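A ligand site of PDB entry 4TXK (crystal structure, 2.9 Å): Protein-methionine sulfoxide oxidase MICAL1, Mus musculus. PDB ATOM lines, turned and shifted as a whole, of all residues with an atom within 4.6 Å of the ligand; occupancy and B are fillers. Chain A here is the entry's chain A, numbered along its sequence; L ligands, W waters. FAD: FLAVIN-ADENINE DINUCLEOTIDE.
An oxygen (O2P) of the ligand sits close to the backbone nitrogen (N) of Pro 94, at 3.4 Å. Merely in contact with the ligand: Val 90 (3.7 Å), Gly 91 (3.3 Å), Ala 92 (3.98 Å), Gly 93 (3.6 Å), Val 113 (3.6 Å), Val 124 (3.7 Å), Leu 125 (3.3 Å), Ile 157 (3.5 Å), Val 179 (3.6 Å), Lys 180 (3.3 Å), Ala 217 (3.6 Å), Ala 218 (3.2 Å), Gly 219 (3.3 Å), Phe 222 (3.9 Å), Thr 241 (3.9 Å), Val 391 (3.97 Å), Gly 392 (3.1 Å), Pro 398 (3.98 Å) and Gly 405 (3.6 Å). Hydrophobic or aromatic side chains that line the ligand: Val 90, Pro 94, Leu 125, Ile 157, Phe 181, Ala 218, Phe 222, Tyr 293, Pro 398 and Trp 400. Of the 35 residues printed, 30 come within 4 Å of the ligand.
The side-chain hydroxyl (OH) of Tyr 293 lies within hydrogen-bond range of an oxygen (O4) of the ligand, 2.5 Å away. An oxygen (O1P) of the ligand lies within hydrogen-bond range of the backbone NH (N) of Asp 393 (2.6 Å). O3' of the ligand lies close to OD1 of Asp 393 (3.5 Å). O2B of the ligand sits at hydrogen-bond distance from OE2 of Glu 114. The side-chain amide nitrogen of Asn 123 is in hydrogen-bond range of a nitrogen (N5) of the ligand, 2.8 Å away. N of Phe 181 sits at hydrogen-bond distance from N1A of the ligand. N6A of the ligand is in hydrogen-bond range of O of Phe 181. An oxygen (O1A) of the ligand is in salt-bridge range of the guanidinium group (NH2) of Arg 121 (3.0 Å). N of Lys 115 lies within hydrogen-bond range of N3A of the ligand, 3.0 Å away. An oxygen (O2B) of the ligand lies within hydrogen-bond range of the guanidinium group of Arg 116 (3.1 Å). An oxygen (O2P) of the ligand is in hydrogen-bond range of the backbone NH of Cys 95 (3.1 Å). The side-chain sulfur (SG) of Cys 95 lies close to an oxygen (O2P) of the ligand (3.3 Å). NE1 of Trp 400 sits at hydrogen-bond distance from N1 of the ligand, 3.2 Å away.
Water W1 bridges the backbone carbonyl oxygen of Trp 400 (2.9 Å) and an oxygen (O2) of the ligand (3.0 Å).
OE2 of Glu 114 is in hydrogen-bond range of N of Arg 116. The backbone carbonyl oxygen (O) of Glu 114 sits at hydrogen-bond distance from the backbone NH (N) of Val 179 (2.8 Å). N of Ala 92 lies within hydrogen-bond range of OE1 of Glu 114. The backbone NH (N) of Ile 157 sits at hydrogen-bond distance from the backbone carbonyl oxygen (O) of Asn 123 (3.0 Å). OG1 of Thr 241 is in hydrogen-bond range of ND2 of Asn 123 (2.8 Å). O of Val 90 is in hydrogen-bond range of N of Ala 218. N of Gly 91 is in hydrogen-bond range of O of Val 113, at 2.9 Å. The backbone carbonyl oxygen (O) of Val 391 lies within hydrogen-bond range of the side-chain sulfur (SG) of Cys 394, 3.5 Å away.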
ATOM      1  N   VAL A  90     -20.431 -20.079 -33.199  1.00  0.00           N
ATOM      2  CA  VAL A  90     -21.376 -19.801 -32.145  1.00  0.00           C
ATOM      3  C   VAL A  90     -21.601 -18.310 -32.026  1.00  0.00           C
ATOM      4  O   VAL A  90     -20.771 -17.595 -31.452  1.00  0.00           O
ATOM      5  CB  VAL A  90     -20.900 -20.373 -30.811  1.00  0.00           C
ATOM      6  CG1 VAL A  90     -22.019 -20.257 -29.790  1.00  0.00           C
ATOM      7  CG2 VAL A  90     -20.484 -21.810 -30.990  1.00  0.00           C
ATOM      8  N   GLY A  91     -22.713 -17.833 -32.588  1.00  0.00           N
ATOM      9  CA  GLY A  91     -23.110 -16.435 -32.432  1.00  0.00           C
ATOM     10  C   GLY A  91     -23.239 -15.634 -33.704  1.00  0.00           C
ATOM     11  O   GLY A  91     -22.307 -15.575 -34.517  1.00  0.00           O
ATOM     12  N   ALA A  92     -24.390 -14.980 -33.865  1.00  0.00           N
ATOM     13  CA  ALA A  92     -24.691 -14.144 -35.047  1.00  0.00           C
ATOM     14  C   ALA A  92     -24.388 -12.671 -34.792  1.00  0.00           C
ATOM     15  O   ALA A  92     -24.929 -11.798 -35.466  1.00  0.00           O
ATOM     16  CB  ALA A  92     -26.175 -14.316 -35.462  1.00  0.00           C
ATOM     17  N   GLY A  93     -23.522 -12.401 -33.826  1.00  0.00           N
ATOM     18  CA  GLY A  93     -23.023 -11.051 -33.640  1.00  0.00           C
ATOM     19  C   GLY A  93     -22.222 -10.700 -34.873  1.00  0.00           C
ATOM     20  O   GLY A  93     -21.950 -11.578 -35.708  1.00  0.00           O
ATOM     21  N   PRO A  94     -21.853  -9.421 -35.019  1.00  0.00           N
ATOM     22  CA  PRO A  94     -21.148  -8.963 -36.207  1.00  0.00           C
ATOM     23  C   PRO A  94     -19.953  -9.839 -36.527  1.00  0.00           C
ATOM     24  O   PRO A  94     -19.744 -10.246 -37.679  1.00  0.00           O
ATOM     25  CB  PRO A  94     -20.709  -7.551 -35.833  1.00  0.00           C
ATOM     26  CG  PRO A  94     -21.733  -7.104 -34.852  1.00  0.00           C
ATOM     27  CD  PRO A  94     -22.065  -8.337 -34.044  1.00  0.00           C
ATOM     28  N   CYS A  95     -19.207 -10.179 -35.478  1.00  0.00           N
ATOM     29  CA  CYS A  95     -17.947 -10.913 -35.600  1.00  0.00           C
ATOM     30  C   CYS A  95     -18.188 -12.349 -35.982  1.00  0.00           C
ATOM     31  O   CYS A  95     -17.406 -12.927 -36.755  1.00  0.00           O
ATOM     32  CB  CYS A  95     -17.179 -10.835 -34.287  1.00  0.00           C
ATOM     33  SG  CYS A  95     -16.851  -9.109 -33.862  1.00  0.00           S
ATOM     34  N   GLY A  96     -19.267 -12.933 -35.468  1.00  0.00           N
ATOM     35  CA  GLY A  96     -19.631 -14.299 -35.797  1.00  0.00           C
ATOM     36  C   GLY A  96     -19.989 -14.378 -37.262  1.00  0.00           C
ATOM     37  O   GLY A  96     -19.453 -15.224 -37.975  1.00  0.00           O
ATOM     38  N   VAL A 113     -25.096 -21.156 -35.076  1.00  0.00           N
ATOM     39  CA  VAL A 113     -26.183 -21.158 -34.098  1.00  0.00           C
ATOM     40  C   VAL A 113     -26.276 -19.804 -33.389  1.00  0.00           C
ATOM     41  O   VAL A 113     -25.261 -19.272 -32.902  1.00  0.00           O
ATOM     42  CB  VAL A 113     -25.998 -22.290 -33.058  1.00  0.00           C
ATOM     43  CG1 VAL A 113     -25.963 -23.647 -33.759  1.00  0.00           C
ATOM     44  CG2 VAL A 113     -24.741 -22.082 -32.218  1.00  0.00           C
ATOM     45  N   GLU A 114     -27.476 -19.230 -33.368  1.00  0.00           N
ATOM     46  CA  GLU A 114     -27.730 -17.981 -32.642  1.00  0.00           C
ATOM     47  C   GLU A 114     -28.809 -18.190 -31.599  1.00  0.00           C
ATOM     48  O   GLU A 114     -29.840 -18.783 -31.877  1.00  0.00           O
ATOM     49  CB  GLU A 114     -28.114 -16.845 -33.593  1.00  0.00           C
ATOM     50  CG  GLU A 114     -28.699 -15.571 -32.929  1.00  0.00           C
ATOM     51  CD  GLU A 114     -27.752 -14.838 -31.935  1.00  0.00           C
ATOM     52  OE1 GLU A 114     -26.582 -14.492 -32.255  1.00  0.00           O
ATOM     53  OE2 GLU A 114     -28.222 -14.599 -30.793  1.00  0.00           O
ATOM     54  N   LYS A 115     -28.519 -17.699 -30.390  1.00  0.00           N
ATOM     55  CA  LYS A 115     -29.410 -17.683 -29.240  1.00  0.00           C
ATOM     56  C   LYS A 115     -30.725 -16.946 -29.470  1.00  0.00           C
ATOM     57  O   LYS A 115     -31.803 -17.437 -29.124  1.00  0.00           O
ATOM     58  CB  LYS A 115     -28.684 -17.022 -28.057  1.00  0.00           C
ATOM     59  CG  LYS A 115     -28.996 -17.639 -26.726  1.00  0.00           C
ATOM     60  CD  LYS A 115     -27.991 -17.236 -25.659  1.00  0.00           C
ATOM     61  CE  LYS A 115     -27.920 -15.755 -25.522  1.00  0.00           C
ATOM     62  NZ  LYS A 115     -27.197 -15.416 -24.285  1.00  0.00           N
ATOM     63  N   ARG A 116     -30.630 -15.751 -30.057  1.00  0.00           N
ATOM     64  CA  ARG A 116     -31.774 -14.862 -30.157  1.00  0.00           C
ATOM     65  C   ARG A 116     -32.496 -15.026 -31.486  1.00  0.00           C
ATOM     66  O   ARG A 116     -32.089 -15.836 -32.330  1.00  0.00           O
ATOM     67  CB  ARG A 116     -31.322 -13.423 -29.963  1.00  0.00           C
ATOM     68  CG  ARG A 116     -30.478 -13.278 -28.719  1.00  0.00           C
ATOM     69  CD  ARG A 116     -30.169 -11.846 -28.371  1.00  0.00           C
ATOM     70  NE  ARG A 116     -29.342 -11.821 -27.174  1.00  0.00           N
ATOM     71  CZ  ARG A 116     -29.822 -11.880 -25.932  1.00  0.00           C
ATOM     72  NH1 ARG A 116     -31.139 -11.974 -25.722  1.00  0.00           N
ATOM     73  NH2 ARG A 116     -28.980 -11.861 -24.898  1.00  0.00           N
ATOM     74  N   ARG A 121     -30.253  -4.667 -30.852  1.00  0.00           N
ATOM     75  CA  ARG A 121     -29.359  -3.683 -30.266  1.00  0.00           C
ATOM     76  C   ARG A 121     -29.174  -2.423 -31.094  1.00  0.00           C
ATOM     77  O   ARG A 121     -28.748  -2.481 -32.240  1.00  0.00           O
ATOM     78  CB  ARG A 121     -27.999  -4.316 -29.990  1.00  0.00           C
ATOM     79  CG  ARG A 121     -28.067  -5.257 -28.838  1.00  0.00           C
ATOM     80  CD  ARG A 121     -26.739  -5.881 -28.564  1.00  0.00           C
ATOM     81  NE  ARG A 121     -26.431  -6.913 -29.539  1.00  0.00           N
ATOM     82  CZ  ARG A 121     -25.232  -7.462 -29.682  1.00  0.00           C
ATOM     83  NH1 ARG A 121     -24.217  -7.055 -28.920  1.00  0.00           N
ATOM     84  NH2 ARG A 121     -25.033  -8.396 -30.603  1.00  0.00           N
ATOM     85  N   ASN A 123     -27.376   0.464 -29.912  1.00  0.00           N
ATOM     86  CA  ASN A 123     -26.154   1.217 -29.616  1.00  0.00           C
ATOM     87  C   ASN A 123     -25.283   1.320 -30.873  1.00  0.00           C
ATOM     88  O   ASN A 123     -25.351   0.448 -31.743  1.00  0.00           O
ATOM     89  CB  ASN A 123     -25.367   0.555 -28.488  1.00  0.00           C
ATOM     90  CG  ASN A 123     -25.894   0.924 -27.113  1.00  0.00           C
ATOM     91  OD1 ASN A 123     -26.941   1.557 -26.985  1.00  0.00           O
ATOM     92  ND2 ASN A 123     -25.161   0.524 -26.082  1.00  0.00           N
ATOM     93  N   VAL A 124     -24.467   2.374 -30.986  1.00  0.00           N
ATOM     94  CA  VAL A 124     -23.702   2.595 -32.212  1.00  0.00           C
ATOM     95  C   VAL A 124     -22.216   2.235 -32.067  1.00  0.00           C
ATOM     96  O   VAL A 124     -21.596   2.568 -31.055  1.00  0.00           O
ATOM     97  CB  VAL A 124     -23.832   4.067 -32.693  1.00  0.00           C
ATOM     98  CG1 VAL A 124     -23.089   4.283 -33.997  1.00  0.00           C
ATOM     99  CG2 VAL A 124     -25.302   4.420 -32.878  1.00  0.00           C
ATOM    100  N   LEU A 125     -21.666   1.564 -33.077  1.00  0.00           N
ATOM    101  CA  LEU A 125     -20.242   1.187 -33.100  1.00  0.00           C
ATOM    102  C   LEU A 125     -19.397   2.088 -33.995  1.00  0.00           C
ATOM    103  O   LEU A 125     -19.709   2.243 -35.181  1.00  0.00           O
ATOM    104  CB  LEU A 125     -20.096  -0.271 -33.576  1.00  0.00           C
ATOM    105  CG  LEU A 125     -21.020  -1.290 -32.886  1.00  0.00           C
ATOM    106  CD1 LEU A 125     -20.825  -2.736 -33.374  1.00  0.00           C
ATOM    107  CD2 LEU A 125     -20.890  -1.207 -31.349  1.00  0.00           C
ATOM    108  N   ILE A 157     -25.459  -1.362 -34.133  1.00  0.00           N
ATOM    109  CA  ILE A 157     -25.221  -2.814 -34.088  1.00  0.00           C
ATOM    110  C   ILE A 157     -26.128  -3.632 -35.029  1.00  0.00           C
ATOM    111  O   ILE A 157     -25.660  -4.297 -35.956  1.00  0.00           O
ATOM    112  CB  ILE A 157     -25.358  -3.348 -32.652  1.00  0.00           C
ATOM    113  CG1 ILE A 157     -24.286  -2.747 -31.744  1.00  0.00           C
ATOM    114  CG2 ILE A 157     -25.266  -4.879 -32.613  1.00  0.00           C
ATOM    115  CD1 ILE A 157     -24.449  -3.135 -30.286  1.00  0.00           C
ATOM    116  N   VAL A 179     -31.361 -20.893 -30.743  1.00  0.00           N
ATOM    117  CA  VAL A 179     -30.705 -22.124 -30.356  1.00  0.00           C
ATOM    118  C   VAL A 179     -29.409 -21.826 -29.646  1.00  0.00           C
ATOM    119  O   VAL A 179     -28.454 -21.378 -30.278  1.00  0.00           O
ATOM    120  CB  VAL A 179     -30.424 -23.020 -31.563  1.00  0.00           C
ATOM    121  CG1 VAL A 179     -29.538 -24.207 -31.156  1.00  0.00           C
ATOM    122  CG2 VAL A 179     -31.741 -23.501 -32.193  1.00  0.00           C
ATOM    123  N   LYS A 180     -29.400 -22.051 -28.337  1.00  0.00           N
ATOM    124  CA  LYS A 180     -28.246 -21.817 -27.490  1.00  0.00           C
ATOM    125  C   LYS A 180     -27.303 -23.032 -27.411  1.00  0.00           C
ATOM    126  O   LYS A 180     -27.727 -24.139 -27.046  1.00  0.00           O
ATOM    127  CB  LYS A 180     -28.672 -21.410 -26.056  1.00  0.00           C
ATOM    128  CG  LYS A 180     -27.500 -20.829 -25.229  1.00  0.00           C
ATOM    129  CD  LYS A 180     -27.874 -20.480 -23.798  1.00  0.00           C
ATOM    130  CE  LYS A 180     -26.680 -19.874 -23.064  1.00  0.00           C
ATOM    131  NZ  LYS A 180     -26.927 -19.787 -21.592  1.00  0.00           N
ATOM    132  N   PHE A 181     -26.027 -22.798 -27.748  1.00  0.00           N
ATOM    133  CA  PHE A 181     -24.918 -23.744 -27.603  1.00  0.00           C
ATOM    134  C   PHE A 181     -24.436 -23.790 -26.151  1.00  0.00           C
ATOM    135  O   PHE A 181     -23.984 -22.781 -25.609  1.00  0.00           O
ATOM    136  CB  PHE A 181     -23.774 -23.323 -28.560  1.00  0.00           C
ATOM    137  CG  PHE A 181     -22.474 -24.087 -28.364  1.00  0.00           C
ATOM    138  CD1 PHE A 181     -22.214 -25.251 -29.093  1.00  0.00           C
ATOM    139  CD2 PHE A 181     -21.492 -23.607 -27.480  1.00  0.00           C
ATOM    140  CE1 PHE A 181     -21.025 -25.935 -28.918  1.00  0.00           C
ATOM    141  CE2 PHE A 181     -20.290 -24.287 -27.306  1.00  0.00           C
ATOM    142  CZ  PHE A 181     -20.051 -25.455 -28.022  1.00  0.00           C
ATOM    143  N   ALA A 217     -18.032 -17.103 -31.023  1.00  0.00           N
ATOM    144  CA  ALA A 217     -18.092 -15.659 -31.145  1.00  0.00           C
ATOM    145  C   ALA A 217     -19.310 -15.128 -30.374  1.00  0.00           C
ATOM    146  O   ALA A 217     -20.146 -14.406 -30.922  1.00  0.00           O
ATOM    147  CB  ALA A 217     -18.133 -15.252 -32.606  1.00  0.00           C
ATOM    148  N   ALA A 218     -19.365 -15.464 -29.089  1.00  0.00           N
ATOM    149  CA  ALA A 218     -20.594 -15.383 -28.306  1.00  0.00           C
ATOM    150  C   ALA A 218     -20.682 -14.169 -27.352  1.00  0.00           C
ATOM    151  O   ALA A 218     -21.507 -14.162 -26.408  1.00  0.00           O
ATOM    152  CB  ALA A 218     -20.770 -16.678 -27.531  1.00  0.00           C
ATOM    153  N   GLY A 219     -19.858 -13.147 -27.584  1.00  0.00           N
ATOM    154  CA  GLY A 219     -19.947 -11.932 -26.787  1.00  0.00           C
ATOM    155  C   GLY A 219     -19.195 -12.029 -25.482  1.00  0.00           C
ATOM    156  O   GLY A 219     -18.767 -13.103 -25.060  1.00  0.00           O
ATOM    157  N   GLY A 220     -19.046 -10.880 -24.834  1.00  0.00           N
ATOM    158  CA  GLY A 220     -18.213 -10.745 -23.639  1.00  0.00           C
ATOM    159  C   GLY A 220     -18.214 -11.846 -22.600  1.00  0.00           C
ATOM    160  O   GLY A 220     -17.172 -12.183 -22.025  1.00  0.00           O
ATOM    161  N   PHE A 222     -19.379 -15.140 -22.728  1.00  0.00           N
ATOM    162  CA  PHE A 222     -19.369 -16.575 -23.013  1.00  0.00           C
ATOM    163  C   PHE A 222     -18.051 -17.091 -23.610  1.00  0.00           C
ATOM    164  O   PHE A 222     -17.527 -16.561 -24.598  1.00  0.00           O
ATOM    165  CB  PHE A 222     -20.515 -16.969 -23.941  1.00  0.00           C
ATOM    166  CG  PHE A 222     -20.724 -18.431 -24.002  1.00  0.00           C
ATOM    167  CD1 PHE A 222     -19.964 -19.213 -24.852  1.00  0.00           C
ATOM    168  CD2 PHE A 222     -21.646 -19.042 -23.175  1.00  0.00           C
ATOM    169  CE1 PHE A 222     -20.132 -20.587 -24.886  1.00  0.00           C
ATOM    170  CE2 PHE A 222     -21.823 -20.407 -23.215  1.00  0.00           C
ATOM    171  CZ  PHE A 222     -21.063 -21.189 -24.065  1.00  0.00           C
ATOM    172  N   THR A 241     -25.091   4.333 -21.751  1.00  0.00           N
ATOM    173  CA  THR A 241     -25.378   4.627 -23.164  1.00  0.00           C
ATOM    174  C   THR A 241     -26.867   4.915 -23.346  1.00  0.00           C
ATOM    175  O   THR A 241     -27.720   4.399 -22.583  1.00  0.00           O
ATOM    176  CB  THR A 241     -24.915   3.487 -24.150  1.00  0.00           C
ATOM    177  OG1 THR A 241     -25.962   2.538 -24.333  1.00  0.00           O
ATOM    178  CG2 THR A 241     -23.692   2.773 -23.645  1.00  0.00           C
ATOM    179  N   TYR A 293     -27.140   8.873 -30.610  1.00  0.00           N
ATOM    180  CA  TYR A 293     -26.528   7.995 -29.632  1.00  0.00           C
ATOM    181  C   TYR A 293     -25.558   8.774 -28.754  1.00  0.00           C
ATOM    182  O   TYR A 293     -24.773   9.590 -29.253  1.00  0.00           O
ATOM    183  CB  TYR A 293     -25.815   6.840 -30.358  1.00  0.00           C
ATOM    184  CG  TYR A 293     -24.891   6.023 -29.498  1.00  0.00           C
ATOM    185  CD1 TYR A 293     -25.355   4.911 -28.812  1.00  0.00           C
ATOM    186  CD2 TYR A 293     -23.552   6.358 -29.409  1.00  0.00           C
ATOM    187  CE1 TYR A 293     -24.501   4.160 -28.033  1.00  0.00           C
ATOM    188  CE2 TYR A 293     -22.693   5.614 -28.627  1.00  0.00           C
ATOM    189  CZ  TYR A 293     -23.170   4.523 -27.940  1.00  0.00           C
ATOM    190  OH  TYR A 293     -22.281   3.799 -27.164  1.00  0.00           O
ATOM    191  N   PHE A 364     -23.614   0.067 -17.980  1.00  0.00           N
ATOM    192  CA  PHE A 364     -22.667  -1.039 -18.083  1.00  0.00           C
ATOM    193  C   PHE A 364     -21.435  -0.820 -17.200  1.00  0.00           C
ATOM    194  O   PHE A 364     -21.114   0.312 -16.813  1.00  0.00           O
ATOM    195  CB  PHE A 364     -22.233  -1.240 -19.540  1.00  0.00           C
ATOM    196  CG  PHE A 364     -23.385  -1.302 -20.503  1.00  0.00           C
ATOM    197  CD1 PHE A 364     -24.022  -2.507 -20.765  1.00  0.00           C
ATOM    198  CD2 PHE A 364     -23.851  -0.150 -21.117  1.00  0.00           C
ATOM    199  CE1 PHE A 364     -25.096  -2.558 -21.633  1.00  0.00           C
ATOM    200  CE2 PHE A 364     -24.932  -0.204 -21.996  1.00  0.00           C
ATOM    201  CZ  PHE A 364     -25.540  -1.406 -22.250  1.00  0.00           C
ATOM    202  N   VAL A 391     -13.468 -15.502 -31.263  1.00  0.00           N
ATOM    203  CA  VAL A 391     -13.604 -14.306 -32.108  1.00  0.00           C
ATOM    204  C   VAL A 391     -14.535 -13.264 -31.440  1.00  0.00           C
ATOM    205  O   VAL A 391     -15.652 -13.586 -31.014  1.00  0.00           O
ATOM    206  CB  VAL A 391     -14.156 -14.657 -33.523  1.00  0.00           C
ATOM    207  CG1 VAL A 391     -14.648 -13.419 -34.248  1.00  0.00           C
ATOM    208  CG2 VAL A 391     -13.134 -15.431 -34.375  1.00  0.00           C
ATOM    209  N   GLY A 392     -14.086 -12.025 -31.335  1.00  0.00           N
ATOM    210  CA  GLY A 392     -14.993 -10.970 -30.891  1.00  0.00           C
ATOM    211  C   GLY A 392     -14.895 -10.519 -29.435  1.00  0.00           C
ATOM    212  O   GLY A 392     -13.807 -10.449 -28.853  1.00  0.00           O
ATOM    213  N   ASP A 393     -16.042 -10.193 -28.858  1.00  0.00           N
ATOM    214  CA  ASP A 393     -16.041  -9.714 -27.474  1.00  0.00           C
ATOM    215  C   ASP A 393     -15.649 -10.826 -26.501  1.00  0.00           C
ATOM    216  O   ASP A 393     -15.316 -10.567 -25.347  1.00  0.00           O
ATOM    217  CB  ASP A 393     -17.415  -9.140 -27.088  1.00  0.00           C
ATOM    218  CG  ASP A 393     -17.717  -7.792 -27.763  1.00  0.00           C
ATOM    219  OD1 ASP A 393     -16.818  -7.252 -28.442  1.00  0.00           O
ATOM    220  OD2 ASP A 393     -18.841  -7.274 -27.602  1.00  0.00           O
ATOM    221  N   CYS A 394     -15.702 -12.073 -26.964  1.00  0.00           N
ATOM    222  CA  CYS A 394     -15.391 -13.192 -26.095  1.00  0.00           C
ATOM    223  C   CYS A 394     -13.892 -13.417 -26.054  1.00  0.00           C
ATOM    224  O   CYS A 394     -13.379 -14.107 -25.168  1.00  0.00           O
ATOM    225  CB  CYS A 394     -16.105 -14.465 -26.561  1.00  0.00           C
ATOM    226  SG  CYS A 394     -15.371 -15.278 -27.976  1.00  0.00           S
ATOM    227  N   PRO A 398     -13.600  -5.116 -25.617  1.00  0.00           N
ATOM    228  CA  PRO A 398     -13.400  -3.829 -26.287  1.00  0.00           C
ATOM    229  C   PRO A 398     -13.672  -2.665 -25.353  1.00  0.00           C
ATOM    230  O   PRO A 398     -14.418  -2.802 -24.392  1.00  0.00           O
ATOM    231  CB  PRO A 398     -14.415  -3.862 -27.415  1.00  0.00           C
ATOM    232  CG  PRO A 398     -15.531  -4.651 -26.862  1.00  0.00           C
ATOM    233  CD  PRO A 398     -14.914  -5.702 -25.961  1.00  0.00           C
ATOM    234  N   TRP A 400     -15.451   0.844 -25.334  1.00  0.00           N
ATOM    235  CA  TRP A 400     -16.446   1.443 -26.225  1.00  0.00           C
ATOM    236  C   TRP A 400     -16.130   2.875 -26.693  1.00  0.00           C
ATOM    237  O   TRP A 400     -16.189   3.121 -27.916  1.00  0.00           O
ATOM    238  CB  TRP A 400     -17.823   1.393 -25.565  1.00  0.00           C
ATOM    239  CG  TRP A 400     -18.343  -0.004 -25.388  1.00  0.00           C
ATOM    240  CD1 TRP A 400     -17.766  -1.161 -25.800  1.00  0.00           C
ATOM    241  CD2 TRP A 400     -19.573  -0.361 -24.759  1.00  0.00           C
ATOM    242  NE1 TRP A 400     -18.547  -2.229 -25.462  1.00  0.00           N
ATOM    243  CE2 TRP A 400     -19.667  -1.763 -24.808  1.00  0.00           C
ATOM    244  CE3 TRP A 400     -20.589   0.358 -24.151  1.00  0.00           C
ATOM    245  CZ2 TRP A 400     -20.751  -2.458 -24.292  1.00  0.00           C
ATOM    246  CZ3 TRP A 400     -21.653  -0.329 -23.622  1.00  0.00           C
ATOM    247  CH2 TRP A 400     -21.727  -1.723 -23.693  1.00  0.00           C
ATOM    248  N   GLY A 405     -13.794  -2.654 -30.562  1.00  0.00           N
ATOM    249  CA  GLY A 405     -14.799  -3.654 -30.902  1.00  0.00           C
ATOM    250  C   GLY A 405     -14.838  -4.231 -32.295  1.00  0.00           C
ATOM    251  O   GLY A 405     -14.362  -5.341 -32.510  1.00  0.00           O
ATOM    252  N   VAL A 406     -15.423  -3.497 -33.238  1.00  0.00           N
ATOM    253  CA  VAL A 406     -15.591  -4.008 -34.589  1.00  0.00           C
ATOM    254  C   VAL A 406     -14.262  -4.382 -35.241  1.00  0.00           C
ATOM    255  O   VAL A 406     -14.103  -5.496 -35.748  1.00  0.00           O
ATOM    256  CB  VAL A 406     -16.289  -3.004 -35.491  1.00  0.00           C
ATOM    257  CG1 VAL A 406     -16.181  -3.455 -36.933  1.00  0.00           C
ATOM    258  CG2 VAL A 406     -17.749  -2.822 -35.085  1.00  0.00           C
HETATM  259  PA  FAD L   1     -21.775  -9.704 -29.533  1.00  0.00           P
HETATM  260  O1A FAD L   1     -22.041  -8.597 -30.539  1.00  0.00           O
HETATM  261  O2A FAD L   1     -21.700  -9.406 -28.037  1.00  0.00           O
HETATM  262  O5B FAD L   1     -22.900 -10.824 -29.791  1.00  0.00           O
HETATM  263  C5B FAD L   1     -22.657 -12.213 -29.692  1.00  0.00           C
HETATM  264  C4B FAD L   1     -23.898 -12.906 -30.260  1.00  0.00           C
HETATM  265  O4B FAD L   1     -23.880 -14.304 -29.973  1.00  0.00           O
HETATM  266  C3B FAD L   1     -25.207 -12.349 -29.688  1.00  0.00           C
HETATM  267  O3B FAD L   1     -26.214 -12.226 -30.716  1.00  0.00           O
HETATM  268  C2B FAD L   1     -25.660 -13.387 -28.707  1.00  0.00           C
HETATM  269  O2B FAD L   1     -27.095 -13.328 -28.684  1.00  0.00           O
HETATM  270  C1B FAD L   1     -25.102 -14.666 -29.314  1.00  0.00           C
HETATM  271  N9A FAD L   1     -24.826 -15.756 -28.334  1.00  0.00           N
HETATM  272  C8A FAD L   1     -24.251 -15.597 -27.132  1.00  0.00           C
HETATM  273  N7A FAD L   1     -24.140 -16.790 -26.474  1.00  0.00           N
HETATM  274  C5A FAD L   1     -24.642 -17.739 -27.272  1.00  0.00           C
HETATM  275  C6A FAD L   1     -24.821 -19.195 -27.176  1.00  0.00           C
HETATM  276  N6A FAD L   1     -24.425 -19.855 -26.055  1.00  0.00           N
HETATM  277  N1A FAD L   1     -25.401 -19.825 -28.231  1.00  0.00           N
HETATM  278  C2A FAD L   1     -25.799 -19.158 -29.337  1.00  0.00           C
HETATM  279  N3A FAD L   1     -25.657 -17.830 -29.491  1.00  0.00           N
HETATM  280  C4A FAD L   1     -25.101 -17.069 -28.503  1.00  0.00           C
HETATM  281  N1  FAD L   1     -19.928  -1.519 -28.239  1.00  0.00           N
HETATM  282  C2  FAD L   1     -19.713  -0.191 -28.416  1.00  0.00           C
HETATM  283  O2  FAD L   1     -18.649   0.215 -28.962  1.00  0.00           O
HETATM  284  N3  FAD L   1     -20.591   0.735 -28.041  1.00  0.00           N
HETATM  285  C4  FAD L   1     -21.751   0.411 -27.451  1.00  0.00           C
HETATM  286  O4  FAD L   1     -22.572   1.289 -27.109  1.00  0.00           O
HETATM  287  C4X FAD L   1     -22.065  -1.008 -27.203  1.00  0.00           C
HETATM  288  N5  FAD L   1     -23.238  -1.389 -26.606  1.00  0.00           N
HETATM  289  C5X FAD L   1     -23.494  -2.701 -26.404  1.00  0.00           C
HETATM  290  C6  FAD L   1     -24.688  -3.111 -25.795  1.00  0.00           C
HETATM  291  C7  FAD L   1     -24.954  -4.468 -25.592  1.00  0.00           C
HETATM  292  C7M FAD L   1     -26.238  -4.896 -24.922  1.00  0.00           C
HETATM  293  C8  FAD L   1     -23.954  -5.488 -26.022  1.00  0.00           C
HETATM  294  C8M FAD L   1     -24.187  -6.960 -25.802  1.00  0.00           C
HETATM  295  C9  FAD L   1     -22.772  -5.086 -26.621  1.00  0.00           C
HETATM  296  C9A FAD L   1     -22.511  -3.737 -26.828  1.00  0.00           C
HETATM  297  N10 FAD L   1     -21.304  -3.348 -27.437  1.00  0.00           N
HETATM  298  C10 FAD L   1     -21.048  -1.983 -27.647  1.00  0.00           C
HETATM  299  C1' FAD L   1     -20.362  -4.371 -27.860  1.00  0.00           C
HETATM  300  C2' FAD L   1     -20.484  -4.582 -29.373  1.00  0.00           C
HETATM  301  O2' FAD L   1     -21.698  -5.238 -29.767  1.00  0.00           O
HETATM  302  C3' FAD L   1     -19.230  -5.335 -29.842  1.00  0.00           C
HETATM  303  O3' FAD L   1     -18.168  -4.339 -29.829  1.00  0.00           O
HETATM  304  C4' FAD L   1     -19.449  -6.025 -31.197  1.00  0.00           C
HETATM  305  O4' FAD L   1     -20.819  -6.432 -31.306  1.00  0.00           O
HETATM  306  C5' FAD L   1     -18.622  -7.280 -31.391  1.00  0.00           C
HETATM  307  O5' FAD L   1     -19.221  -8.249 -30.534  1.00  0.00           O
HETATM  308  P   FAD L   1     -19.322  -9.817 -30.937  1.00  0.00           P
HETATM  309  O1P FAD L   1     -18.048 -10.479 -30.425  1.00  0.00           O
HETATM  310  O2P FAD L   1     -19.723  -9.899 -32.387  1.00  0.00           O
HETATM  311  O3P FAD L   1     -20.462 -10.510 -30.027  1.00  0.00           O
HETATM  312  O   HOH W   1     -17.467   2.597 -30.449  1.00  0.00           O
